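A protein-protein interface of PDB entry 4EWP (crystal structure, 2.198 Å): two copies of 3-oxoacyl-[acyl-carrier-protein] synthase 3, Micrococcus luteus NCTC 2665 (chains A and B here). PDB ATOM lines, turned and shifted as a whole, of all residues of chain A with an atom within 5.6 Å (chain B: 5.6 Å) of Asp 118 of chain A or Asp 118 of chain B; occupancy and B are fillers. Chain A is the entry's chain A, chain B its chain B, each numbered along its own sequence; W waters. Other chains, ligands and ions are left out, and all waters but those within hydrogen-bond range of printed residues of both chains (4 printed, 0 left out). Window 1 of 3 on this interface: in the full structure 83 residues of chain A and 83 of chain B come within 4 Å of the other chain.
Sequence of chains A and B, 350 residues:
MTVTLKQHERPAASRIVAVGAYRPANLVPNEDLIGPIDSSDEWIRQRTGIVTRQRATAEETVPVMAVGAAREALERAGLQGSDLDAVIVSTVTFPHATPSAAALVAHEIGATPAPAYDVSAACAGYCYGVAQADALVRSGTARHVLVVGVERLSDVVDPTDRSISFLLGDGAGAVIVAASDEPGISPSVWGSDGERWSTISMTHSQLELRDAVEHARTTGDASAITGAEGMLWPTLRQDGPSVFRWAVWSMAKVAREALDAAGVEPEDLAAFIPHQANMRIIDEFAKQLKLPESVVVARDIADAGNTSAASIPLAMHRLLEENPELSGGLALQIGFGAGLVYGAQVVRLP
Of the 16 printed residues of chain A, 5 touch a printed residue of chain B.
Hydrophobic or aromatic side chains of chain A that line the printed part of chain B: Tyr 117.
Among the printed residues, 9 pairs touch across the chains.
Ser 90 of chain A touches none of the printed residues of chain B.
Of the printed residues of chain B, Asp 118 of chain A touches Asp 118, Val 119 and Ser 120.
Of the printed residues of chain B, Val 119 of chain A touches Asp 118 (3.4 Å).
Of the printed residues of chain B, Ser 120 of chain A touches Ser 100 (3.6 Å), Tyr 117 (3.6 Å) and Asp 118 (2.9 Å).
Of the printed residues of chain A, Ser 100 of chain B touches Ser 120.
Printed residues of chain A within 4 Å of Tyr 117 of chain B: Ser 120 (3.6 Å).
Of the printed residues of chain A, Ser 120 of chain B touches Ser 100 (3.6 Å), Tyr 117 (3.5 Å) and Asp 118 (2.8 Å).
The nearest printed residue of chain A that does not touch Asp 118 of chain B is Ala 121 of chain A (5.6 Å).
O of Asp 118 of chain A sits at hydrogen-bond distance from N of Ser 120 of chain B (2.8 Å).
The backbone carbonyl oxygen (O) of Asp 118 of chain B sits at hydrogen-bond distance from the backbone NH (N) of Ser 120 of chain A.
Water W2 lies within hydrogen-bond range of O of Ala 116 of chain A, O of Ser 120 of chain B and OG of Ser 100 of chain A.
Water W4 lies within hydrogen-bond range of the backbone carbonyl oxygen of Ser 120 of chain A (2.7 Å), the backbone carbonyl oxygen of Ala 116 of chain B (2.8 Å) and the side-chain hydroxyl of Ser 100 of chain B (2.8 Å).
Water W1 lies within hydrogen-bond range of the backbone carbonyl oxygen of Asp 118 of chain B (3.1 Å), the backbone carbonyl oxygen of Asp 118 of chain A (3.3 Å), the backbone NH of Ser 120 of chain B (3.4 Å) and the backbone NH of Ser 120 of chain A (3.4 Å).
Water W3 lies within hydrogen-bond range of the side-chain hydroxyl (OG) of Ser 120 of chain A (3.1 Å) and the backbone carbonyl oxygen (O) of Pro 99 of chain B (3.3 Å).
The side-chain carboxylate of Asp 118 of chain B lies within hydrogen-bond range of the backbone NH of Ala 101 of chain B (3.0 Å).
OG of Ser 100 of chain B is in hydrogen-bond range of N of Ala 103 of chain B, 3.1 Å away.
The backbone NH (N) of Ala 102 of chain A sits at hydrogen-bond distance from the side-chain carboxylate (OD1) of Asp 118 of chain A, 2.8 Å away.
The side-chain carboxylate (OD1) of Asp 118 of chain B sits at hydrogen-bond distance from the backbone NH (N) of Ala 102 of chain B (2.9 Å).
The backbone carbonyl oxygen (O) of Val 119 of chain B is in hydrogen-bond range of the backbone NH (N) of Thr 91 of chain B, 3.4 Å away.
N of Val 89 of chain B lies within hydrogen-bond range of O of Tyr 117 of chain B (3.1 Å).
Among the printed residues, pairs that only touch across the chains: Ser 100 of chain A with Ser 120 of chain B, Tyr 117 of chain A with Ser 120 of chain B, Asp 118 of chain A with Asp 118 of chain B, Asp 118 of chain A with Val 119 of chain B, Val 119 of chain A with Asp 118 of chain B, Ser 120 of chain A with Ser 100 of chain B and Ser 120 of chain A with Tyr 117 of chain B.
Ser 100 of chain A touches Ser 120 of chain B, and with the chains exchanged Ser 120 of chain A touches Ser 100 of chain B.
Tyr 117 of chain A touches Ser 120 of chain B, and with the chains exchanged Ser 120 of chain A touches Tyr 117 of chain B.
Asp 118 of chain A touches its own counterpart, Asp 118 of chain B.
Asp 118 of chain A touches Val 119 of chain B, and with the chains exchanged Val 119 of chain A touches Asp 118 of chain B.
Positions printed for both chains: 89, 90, 91, 94, 99, 100, 101, 102, 103, 116, 117, 118, 119 and 120.
Of the 9 pairs that touch across the chains among the printed residues, 9 have their exchanged pair printed and touching as well.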
ATOM      1  N   ILE A  88     -12.175  -2.567  22.971  1.00  0.00           N
ATOM      2  CA  ILE A  88     -11.936  -1.946  21.673  1.00  0.00           C
ATOM      3  C   ILE A  88     -12.873  -2.565  20.656  1.00  0.00           C
ATOM      4  O   ILE A  88     -12.877  -3.785  20.450  1.00  0.00           O
ATOM      5  CB  ILE A  88     -10.482  -2.142  21.187  1.00  0.00           C
ATOM      6  CG1 ILE A  88      -9.491  -1.612  22.219  1.00  0.00           C
ATOM      7  CG2 ILE A  88     -10.267  -1.450  19.858  1.00  0.00           C
ATOM      8  CD1 ILE A  88      -8.038  -1.809  21.827  1.00  0.00           C
ATOM      9  N   VAL A  89     -13.688  -1.730  20.031  1.00  0.00           N
ATOM     10  CA  VAL A  89     -14.635  -2.234  19.050  1.00  0.00           C
ATOM     11  C   VAL A  89     -14.279  -1.681  17.681  1.00  0.00           C
ATOM     12  O   VAL A  89     -14.268  -0.467  17.457  1.00  0.00           O
ATOM     13  CB  VAL A  89     -16.082  -1.869  19.396  1.00  0.00           C
ATOM     14  CG1 VAL A  89     -16.979  -2.136  18.193  1.00  0.00           C
ATOM     15  CG2 VAL A  89     -16.541  -2.622  20.645  1.00  0.00           C
ATOM     16  N   SER A  90     -13.967  -2.580  16.765  1.00  0.00           N
ATOM     17  CA  SER A  90     -13.570  -2.160  15.443  1.00  0.00           C
ATOM     18  C   SER A  90     -14.723  -2.368  14.475  1.00  0.00           C
ATOM     19  O   SER A  90     -15.064  -3.497  14.151  1.00  0.00           O
ATOM     20  CB  SER A  90     -12.328  -2.923  15.022  1.00  0.00           C
ATOM     21  OG  SER A  90     -12.128  -2.750  13.645  1.00  0.00           O
ATOM     22  N   THR A  91     -15.329  -1.268  14.031  1.00  0.00           N
ATOM     23  CA  THR A  91     -16.522  -1.318  13.196  1.00  0.00           C
ATOM     24  C   THR A  91     -16.692  -0.016  12.426  1.00  0.00           C
ATOM     25  O   THR A  91     -16.269   1.037  12.893  1.00  0.00           O
ATOM     26  CB  THR A  91     -17.783  -1.505  14.056  1.00  0.00           C
ATOM     27  OG1 THR A  91     -18.938  -1.583  13.214  1.00  0.00           O
ATOM     28  CG2 THR A  91     -17.973  -0.325  14.986  1.00  0.00           C
ATOM     29  N   PHE A  94     -21.813   0.970  12.736  1.00  0.00           N
ATOM     30  CA  PHE A  94     -22.668   1.438  13.820  1.00  0.00           C
ATOM     31  C   PHE A  94     -23.210   2.811  13.413  1.00  0.00           C
ATOM     32  O   PHE A  94     -22.440   3.744  13.193  1.00  0.00           O
ATOM     33  CB  PHE A  94     -21.855   1.505  15.111  1.00  0.00           C
ATOM     34  CG  PHE A  94     -22.662   1.828  16.355  1.00  0.00           C
ATOM     35  CD1 PHE A  94     -22.323   2.926  17.151  1.00  0.00           C
ATOM     36  CD2 PHE A  94     -23.712   1.016  16.757  1.00  0.00           C
ATOM     37  CE1 PHE A  94     -23.023   3.205  18.327  1.00  0.00           C
ATOM     38  CE2 PHE A  94     -24.423   1.294  17.922  1.00  0.00           C
ATOM     39  CZ  PHE A  94     -24.078   2.382  18.713  1.00  0.00           C
ATOM     40  N   PRO A  99     -22.601   8.433  20.761  1.00  0.00           N
ATOM     41  CA  PRO A  99     -21.352   7.865  21.287  1.00  0.00           C
ATOM     42  C   PRO A  99     -21.015   6.524  20.637  1.00  0.00           C
ATOM     43  O   PRO A  99     -21.735   6.064  19.761  1.00  0.00           O
ATOM     44  CB  PRO A  99     -21.648   7.661  22.780  1.00  0.00           C
ATOM     45  CG  PRO A  99     -23.127   8.025  22.995  1.00  0.00           C
ATOM     46  CD  PRO A  99     -23.756   8.218  21.656  1.00  0.00           C
ATOM     47  N   SER A 100     -19.932   5.894  21.077  1.00  0.00           N
ATOM     48  CA  SER A 100     -19.456   4.686  20.434  1.00  0.00           C
ATOM     49  C   SER A 100     -20.314   3.462  20.773  1.00  0.00           C
ATOM     50  O   SER A 100     -21.107   3.466  21.710  1.00  0.00           O
ATOM     51  CB  SER A 100     -18.028   4.410  20.872  1.00  0.00           C
ATOM     52  OG  SER A 100     -18.009   4.122  22.260  1.00  0.00           O
ATOM     53  N   ALA A 101     -20.124   2.407  19.996  1.00  0.00           N
ATOM     54  CA  ALA A 101     -20.763   1.131  20.243  1.00  0.00           C
ATOM     55  C   ALA A 101     -20.075   0.470  21.434  1.00  0.00           C
ATOM     56  O   ALA A 101     -20.702  -0.223  22.242  1.00  0.00           O
ATOM     57  CB  ALA A 101     -20.615   0.267  19.013  1.00  0.00           C
ATOM     58  N   ALA A 102     -18.768   0.699  21.522  1.00  0.00           N
ATOM     59  CA  ALA A 102     -17.937   0.096  22.543  1.00  0.00           C
ATOM     60  C   ALA A 102     -18.488   0.378  23.929  1.00  0.00           C
ATOM     61  O   ALA A 102     -18.420  -0.474  24.828  1.00  0.00           O
ATOM     62  CB  ALA A 102     -16.490   0.609  22.421  1.00  0.00           C
ATOM     63  N   ALA A 103     -19.015   1.583  24.109  1.00  0.00           N
ATOM     64  CA  ALA A 103     -19.491   1.999  25.425  1.00  0.00           C
ATOM     65  C   ALA A 103     -20.727   1.204  25.801  1.00  0.00           C
ATOM     66  O   ALA A 103     -20.891   0.829  26.964  1.00  0.00           O
ATOM     67  CB  ALA A 103     -19.767   3.519  25.461  1.00  0.00           C
ATOM     68  N   ALA A 116     -13.596   2.428  26.819  1.00  0.00           N
ATOM     69  CA  ALA A 116     -14.260   1.757  25.725  1.00  0.00           C
ATOM     70  C   ALA A 116     -14.284   2.725  24.567  1.00  0.00           C
ATOM     71  O   ALA A 116     -14.745   3.859  24.729  1.00  0.00           O
ATOM     72  CB  ALA A 116     -15.685   1.406  26.140  1.00  0.00           C
ATOM     73  N   TYR A 117     -13.791   2.301  23.404  1.00  0.00           N
ATOM     74  CA  TYR A 117     -13.850   3.153  22.210  1.00  0.00           C
ATOM     75  C   TYR A 117     -13.974   2.334  20.935  1.00  0.00           C
ATOM     76  O   TYR A 117     -13.577   1.167  20.908  1.00  0.00           O
ATOM     77  CB  TYR A 117     -12.618   4.061  22.122  1.00  0.00           C
ATOM     78  CG  TYR A 117     -11.263   3.358  21.998  1.00  0.00           C
ATOM     79  CD1 TYR A 117     -10.637   3.205  20.766  1.00  0.00           C
ATOM     80  CD2 TYR A 117     -10.596   2.893  23.124  1.00  0.00           C
ATOM     81  CE1 TYR A 117      -9.386   2.583  20.668  1.00  0.00           C
ATOM     82  CE2 TYR A 117      -9.361   2.283  23.031  1.00  0.00           C
ATOM     83  CZ  TYR A 117      -8.760   2.136  21.815  1.00  0.00           C
ATOM     84  OH  TYR A 117      -7.532   1.532  21.751  1.00  0.00           O
ATOM     85  N   ASP A 118     -14.520   2.946  19.887  1.00  0.00           N
ATOM     86  CA  ASP A 118     -14.578   2.318  18.567  1.00  0.00           C
ATOM     87  C   ASP A 118     -13.380   2.797  17.766  1.00  0.00           C
ATOM     88  O   ASP A 118     -12.877   3.902  17.993  1.00  0.00           O
ATOM     89  CB  ASP A 118     -15.841   2.718  17.795  1.00  0.00           C
ATOM     90  CG  ASP A 118     -17.128   2.217  18.440  1.00  0.00           C
ATOM     91  OD1 ASP A 118     -17.077   1.459  19.446  1.00  0.00           O
ATOM     92  OD2 ASP A 118     -18.209   2.590  17.924  1.00  0.00           O
ATOM     93  N   VAL A 119     -12.945   1.962  16.826  1.00  0.00           N
ATOM     94  CA  VAL A 119     -11.821   2.245  15.948  1.00  0.00           C
ATOM     95  C   VAL A 119     -12.297   2.162  14.497  1.00  0.00           C
ATOM     96  O   VAL A 119     -13.157   1.345  14.167  1.00  0.00           O
ATOM     97  CB  VAL A 119     -10.698   1.209  16.160  1.00  0.00           C
ATOM     98  CG1 VAL A 119      -9.856   1.056  14.918  1.00  0.00           C
ATOM     99  CG2 VAL A 119      -9.844   1.591  17.348  1.00  0.00           C
ATOM    100  N   SER A 120     -11.770   3.027  13.640  1.00  0.00           N
ATOM    101  CA  SER A 120     -12.105   2.981  12.225  1.00  0.00           C
ATOM    102  C   SER A 120     -10.870   2.617  11.411  1.00  0.00           C
ATOM    103  O   SER A 120     -10.001   3.471  11.157  1.00  0.00           O
ATOM    104  CB  SER A 120     -12.661   4.319  11.735  1.00  0.00           C
ATOM    105  OG  SER A 120     -13.052   4.241  10.367  1.00  0.00           O
ATOM    106  N   ALA A 121     -10.813   1.352  10.999  1.00  0.00           N
ATOM    107  CA  ALA A 121      -9.720   0.849  10.181  1.00  0.00           C
ATOM    108  C   ALA A 121     -10.225  -0.253   9.259  1.00  0.00           C
ATOM    109  O   ALA A 121      -9.487  -1.199   8.893  1.00  0.00           O
ATOM    110  CB  ALA A 121      -8.587   0.366  11.055  1.00  0.00           C
ATOM    111  N   VAL B  89      -6.615   9.863  14.906  1.00  0.00           N
ATOM    112  CA  VAL B  89      -7.523  11.004  14.816  1.00  0.00           C
ATOM    113  C   VAL B  89      -8.786  10.745  15.638  1.00  0.00           C
ATOM    114  O   VAL B  89      -9.515   9.786  15.371  1.00  0.00           O
ATOM    115  CB  VAL B  89      -7.933  11.324  13.365  1.00  0.00           C
ATOM    116  CG1 VAL B  89      -9.084  12.335  13.355  1.00  0.00           C
ATOM    117  CG2 VAL B  89      -6.747  11.828  12.573  1.00  0.00           C
ATOM    118  N   SER B  90      -9.041  11.596  16.633  1.00  0.00           N
ATOM    119  CA  SER B  90     -10.240  11.444  17.443  1.00  0.00           C
ATOM    120  C   SER B  90     -11.270  12.446  16.982  1.00  0.00           C
ATOM    121  O   SER B  90     -11.075  13.669  17.132  1.00  0.00           O
ATOM    122  CB  SER B  90      -9.935  11.615  18.930  1.00  0.00           C
ATOM    123  OG  SER B  90      -8.903  10.708  19.296  1.00  0.00           O
ATOM    124  N   THR B  91     -12.350  11.929  16.392  1.00  0.00           N
ATOM    125  CA  THR B  91     -13.385  12.767  15.780  1.00  0.00           C
ATOM    126  C   THR B  91     -14.647  11.947  15.697  1.00  0.00           C
ATOM    127  O   THR B  91     -14.584  10.716  15.603  1.00  0.00           O
ATOM    128  CB  THR B  91     -12.996  13.209  14.340  1.00  0.00           C
ATOM    129  OG1 THR B  91     -14.027  14.048  13.779  1.00  0.00           O
ATOM    130  CG2 THR B  91     -12.815  11.993  13.438  1.00  0.00           C
ATOM    131  N   PHE B  94     -16.507  13.233  11.070  1.00  0.00           N
ATOM    132  CA  PHE B  94     -16.091  12.948   9.690  1.00  0.00           C
ATOM    133  C   PHE B  94     -17.231  12.223   8.955  1.00  0.00           C
ATOM    134  O   PHE B  94     -17.637  11.141   9.364  1.00  0.00           O
ATOM    135  CB  PHE B  94     -14.802  12.132   9.674  1.00  0.00           C
ATOM    136  CG  PHE B  94     -14.190  11.989   8.312  1.00  0.00           C
ATOM    137  CD1 PHE B  94     -13.890  10.730   7.807  1.00  0.00           C
ATOM    138  CD2 PHE B  94     -13.933  13.110   7.529  1.00  0.00           C
ATOM    139  CE1 PHE B  94     -13.336  10.582   6.548  1.00  0.00           C
ATOM    140  CE2 PHE B  94     -13.365  12.977   6.262  1.00  0.00           C
ATOM    141  CZ  PHE B  94     -13.063  11.714   5.773  1.00  0.00           C
ATOM    142  N   PRO B  99     -13.564   5.059   4.257  1.00  0.00           N
ATOM    143  CA  PRO B  99     -12.435   4.846   5.160  1.00  0.00           C
ATOM    144  C   PRO B  99     -12.293   6.012   6.146  1.00  0.00           C
ATOM    145  O   PRO B  99     -13.108   6.937   6.169  1.00  0.00           O
ATOM    146  CB  PRO B  99     -11.219   4.840   4.226  1.00  0.00           C
ATOM    147  CG  PRO B  99     -11.760   4.993   2.808  1.00  0.00           C
ATOM    148  CD  PRO B  99     -13.135   5.525   2.924  1.00  0.00           C
ATOM    149  N   SER B 100     -11.225   5.981   6.931  1.00  0.00           N
ATOM    150  CA  SER B 100     -11.039   6.949   8.000  1.00  0.00           C
ATOM    151  C   SER B 100     -10.479   8.295   7.517  1.00  0.00           C
ATOM    152  O   SER B 100      -9.901   8.404   6.438  1.00  0.00           O
ATOM    153  CB  SER B 100     -10.108   6.369   9.062  1.00  0.00           C
ATOM    154  OG  SER B 100      -8.805   6.179   8.535  1.00  0.00           O
ATOM    155  N   ALA B 101     -10.655   9.309   8.350  1.00  0.00           N
ATOM    156  CA  ALA B 101     -10.022  10.608   8.159  1.00  0.00           C
ATOM    157  C   ALA B 101      -8.505  10.490   8.366  1.00  0.00           C
ATOM    158  O   ALA B 101      -7.715  11.147   7.685  1.00  0.00           O
ATOM    159  CB  ALA B 101     -10.616  11.596   9.149  1.00  0.00           C
ATOM    160  N   ALA B 102      -8.112   9.634   9.307  1.00  0.00           N
ATOM    161  CA  ALA B 102      -6.706   9.412   9.628  1.00  0.00           C
ATOM    162  C   ALA B 102      -5.922   8.971   8.393  1.00  0.00           C
ATOM    163  O   ALA B 102      -4.768   9.380   8.191  1.00  0.00           O
ATOM    164  CB  ALA B 102      -6.581   8.342  10.735  1.00  0.00           C
ATOM    165  N   ALA B 103      -6.542   8.123   7.570  1.00  0.00           N
ATOM    166  CA  ALA B 103      -5.867   7.638   6.369  1.00  0.00           C
ATOM    167  C   ALA B 103      -5.555   8.817   5.430  1.00  0.00           C
ATOM    168  O   ALA B 103      -4.480   8.871   4.821  1.00  0.00           O
ATOM    169  CB  ALA B 103      -6.709   6.567   5.670  1.00  0.00           C
ATOM    170  N   ALA B 116      -2.807   4.319  10.579  1.00  0.00           N
ATOM    171  CA  ALA B 116      -3.649   5.488  10.799  1.00  0.00           C
ATOM    172  C   ALA B 116      -5.080   5.023  11.027  1.00  0.00           C
ATOM    173  O   ALA B 116      -5.608   4.234  10.237  1.00  0.00           O
ATOM    174  CB  ALA B 116      -3.588   6.399   9.562  1.00  0.00           C
ATOM    175  N   TYR B 117      -5.706   5.502  12.095  1.00  0.00           N
ATOM    176  CA  TYR B 117      -7.077   5.121  12.394  1.00  0.00           C
ATOM    177  C   TYR B 117      -7.812   6.241  13.142  1.00  0.00           C
ATOM    178  O   TYR B 117      -7.174   7.067  13.816  1.00  0.00           O
ATOM    179  CB  TYR B 117      -7.106   3.801  13.191  1.00  0.00           C
ATOM    180  CG  TYR B 117      -6.401   3.825  14.545  1.00  0.00           C
ATOM    181  CD1 TYR B 117      -7.105   4.120  15.708  1.00  0.00           C
ATOM    182  CD2 TYR B 117      -5.058   3.515  14.665  1.00  0.00           C
ATOM    183  CE1 TYR B 117      -6.492   4.111  16.953  1.00  0.00           C
ATOM    184  CE2 TYR B 117      -4.432   3.493  15.905  1.00  0.00           C
ATOM    185  CZ  TYR B 117      -5.160   3.802  17.048  1.00  0.00           C
ATOM    186  OH  TYR B 117      -4.576   3.808  18.291  1.00  0.00           O
ATOM    187  N   ASP B 118      -9.138   6.272  12.998  1.00  0.00           N
ATOM    188  CA  ASP B 118     -10.003   7.178  13.760  1.00  0.00           C
ATOM    189  C   ASP B 118     -10.471   6.502  15.034  1.00  0.00           C
ATOM    190  O   ASP B 118     -10.768   5.297  15.048  1.00  0.00           O
ATOM    191  CB  ASP B 118     -11.257   7.578  12.969  1.00  0.00           C
ATOM    192  CG  ASP B 118     -10.964   8.521  11.806  1.00  0.00           C
ATOM    193  OD1 ASP B 118      -9.791   8.929  11.614  1.00  0.00           O
ATOM    194  OD2 ASP B 118     -11.933   8.847  11.078  1.00  0.00           O
ATOM    195  N   VAL B 119     -10.553   7.279  16.104  1.00  0.00           N
ATOM    196  CA  VAL B 119     -11.030   6.766  17.374  1.00  0.00           C
ATOM    197  C   VAL B 119     -12.341   7.455  17.691  1.00  0.00           C
ATOM    198  O   VAL B 119     -12.473   8.660  17.451  1.00  0.00           O
ATOM    199  CB  VAL B 119     -10.028   7.081  18.475  1.00  0.00           C
ATOM    200  CG1 VAL B 119     -10.708   7.149  19.831  1.00  0.00           C
ATOM    201  CG2 VAL B 119      -8.886   6.071  18.459  1.00  0.00           C
ATOM    202  N   SER B 120     -13.305   6.709  18.232  1.00  0.00           N
ATOM    203  CA  SER B 120     -14.572   7.296  18.666  1.00  0.00           C
ATOM    204  C   SER B 120     -14.724   7.322  20.193  1.00  0.00           C
ATOM    205  O   SER B 120     -15.014   6.292  20.824  1.00  0.00           O
ATOM    206  CB  SER B 120     -15.764   6.583  18.021  1.00  0.00           C
ATOM    207  OG  SER B 120     -16.989   7.195  18.418  1.00  0.00           O
HETATM  208  O   HOH W   1     -13.823   5.296  15.205  1.00  0.00           O
HETATM  209  O   HOH W   2     -15.937   5.742  23.337  1.00  0.00           O
HETATM  210  O   HOH W   3     -14.312   6.835   9.240  1.00  0.00           O
HETATM  211  O   HOH W   4      -8.113   3.543   9.211  1.00  0.00           O
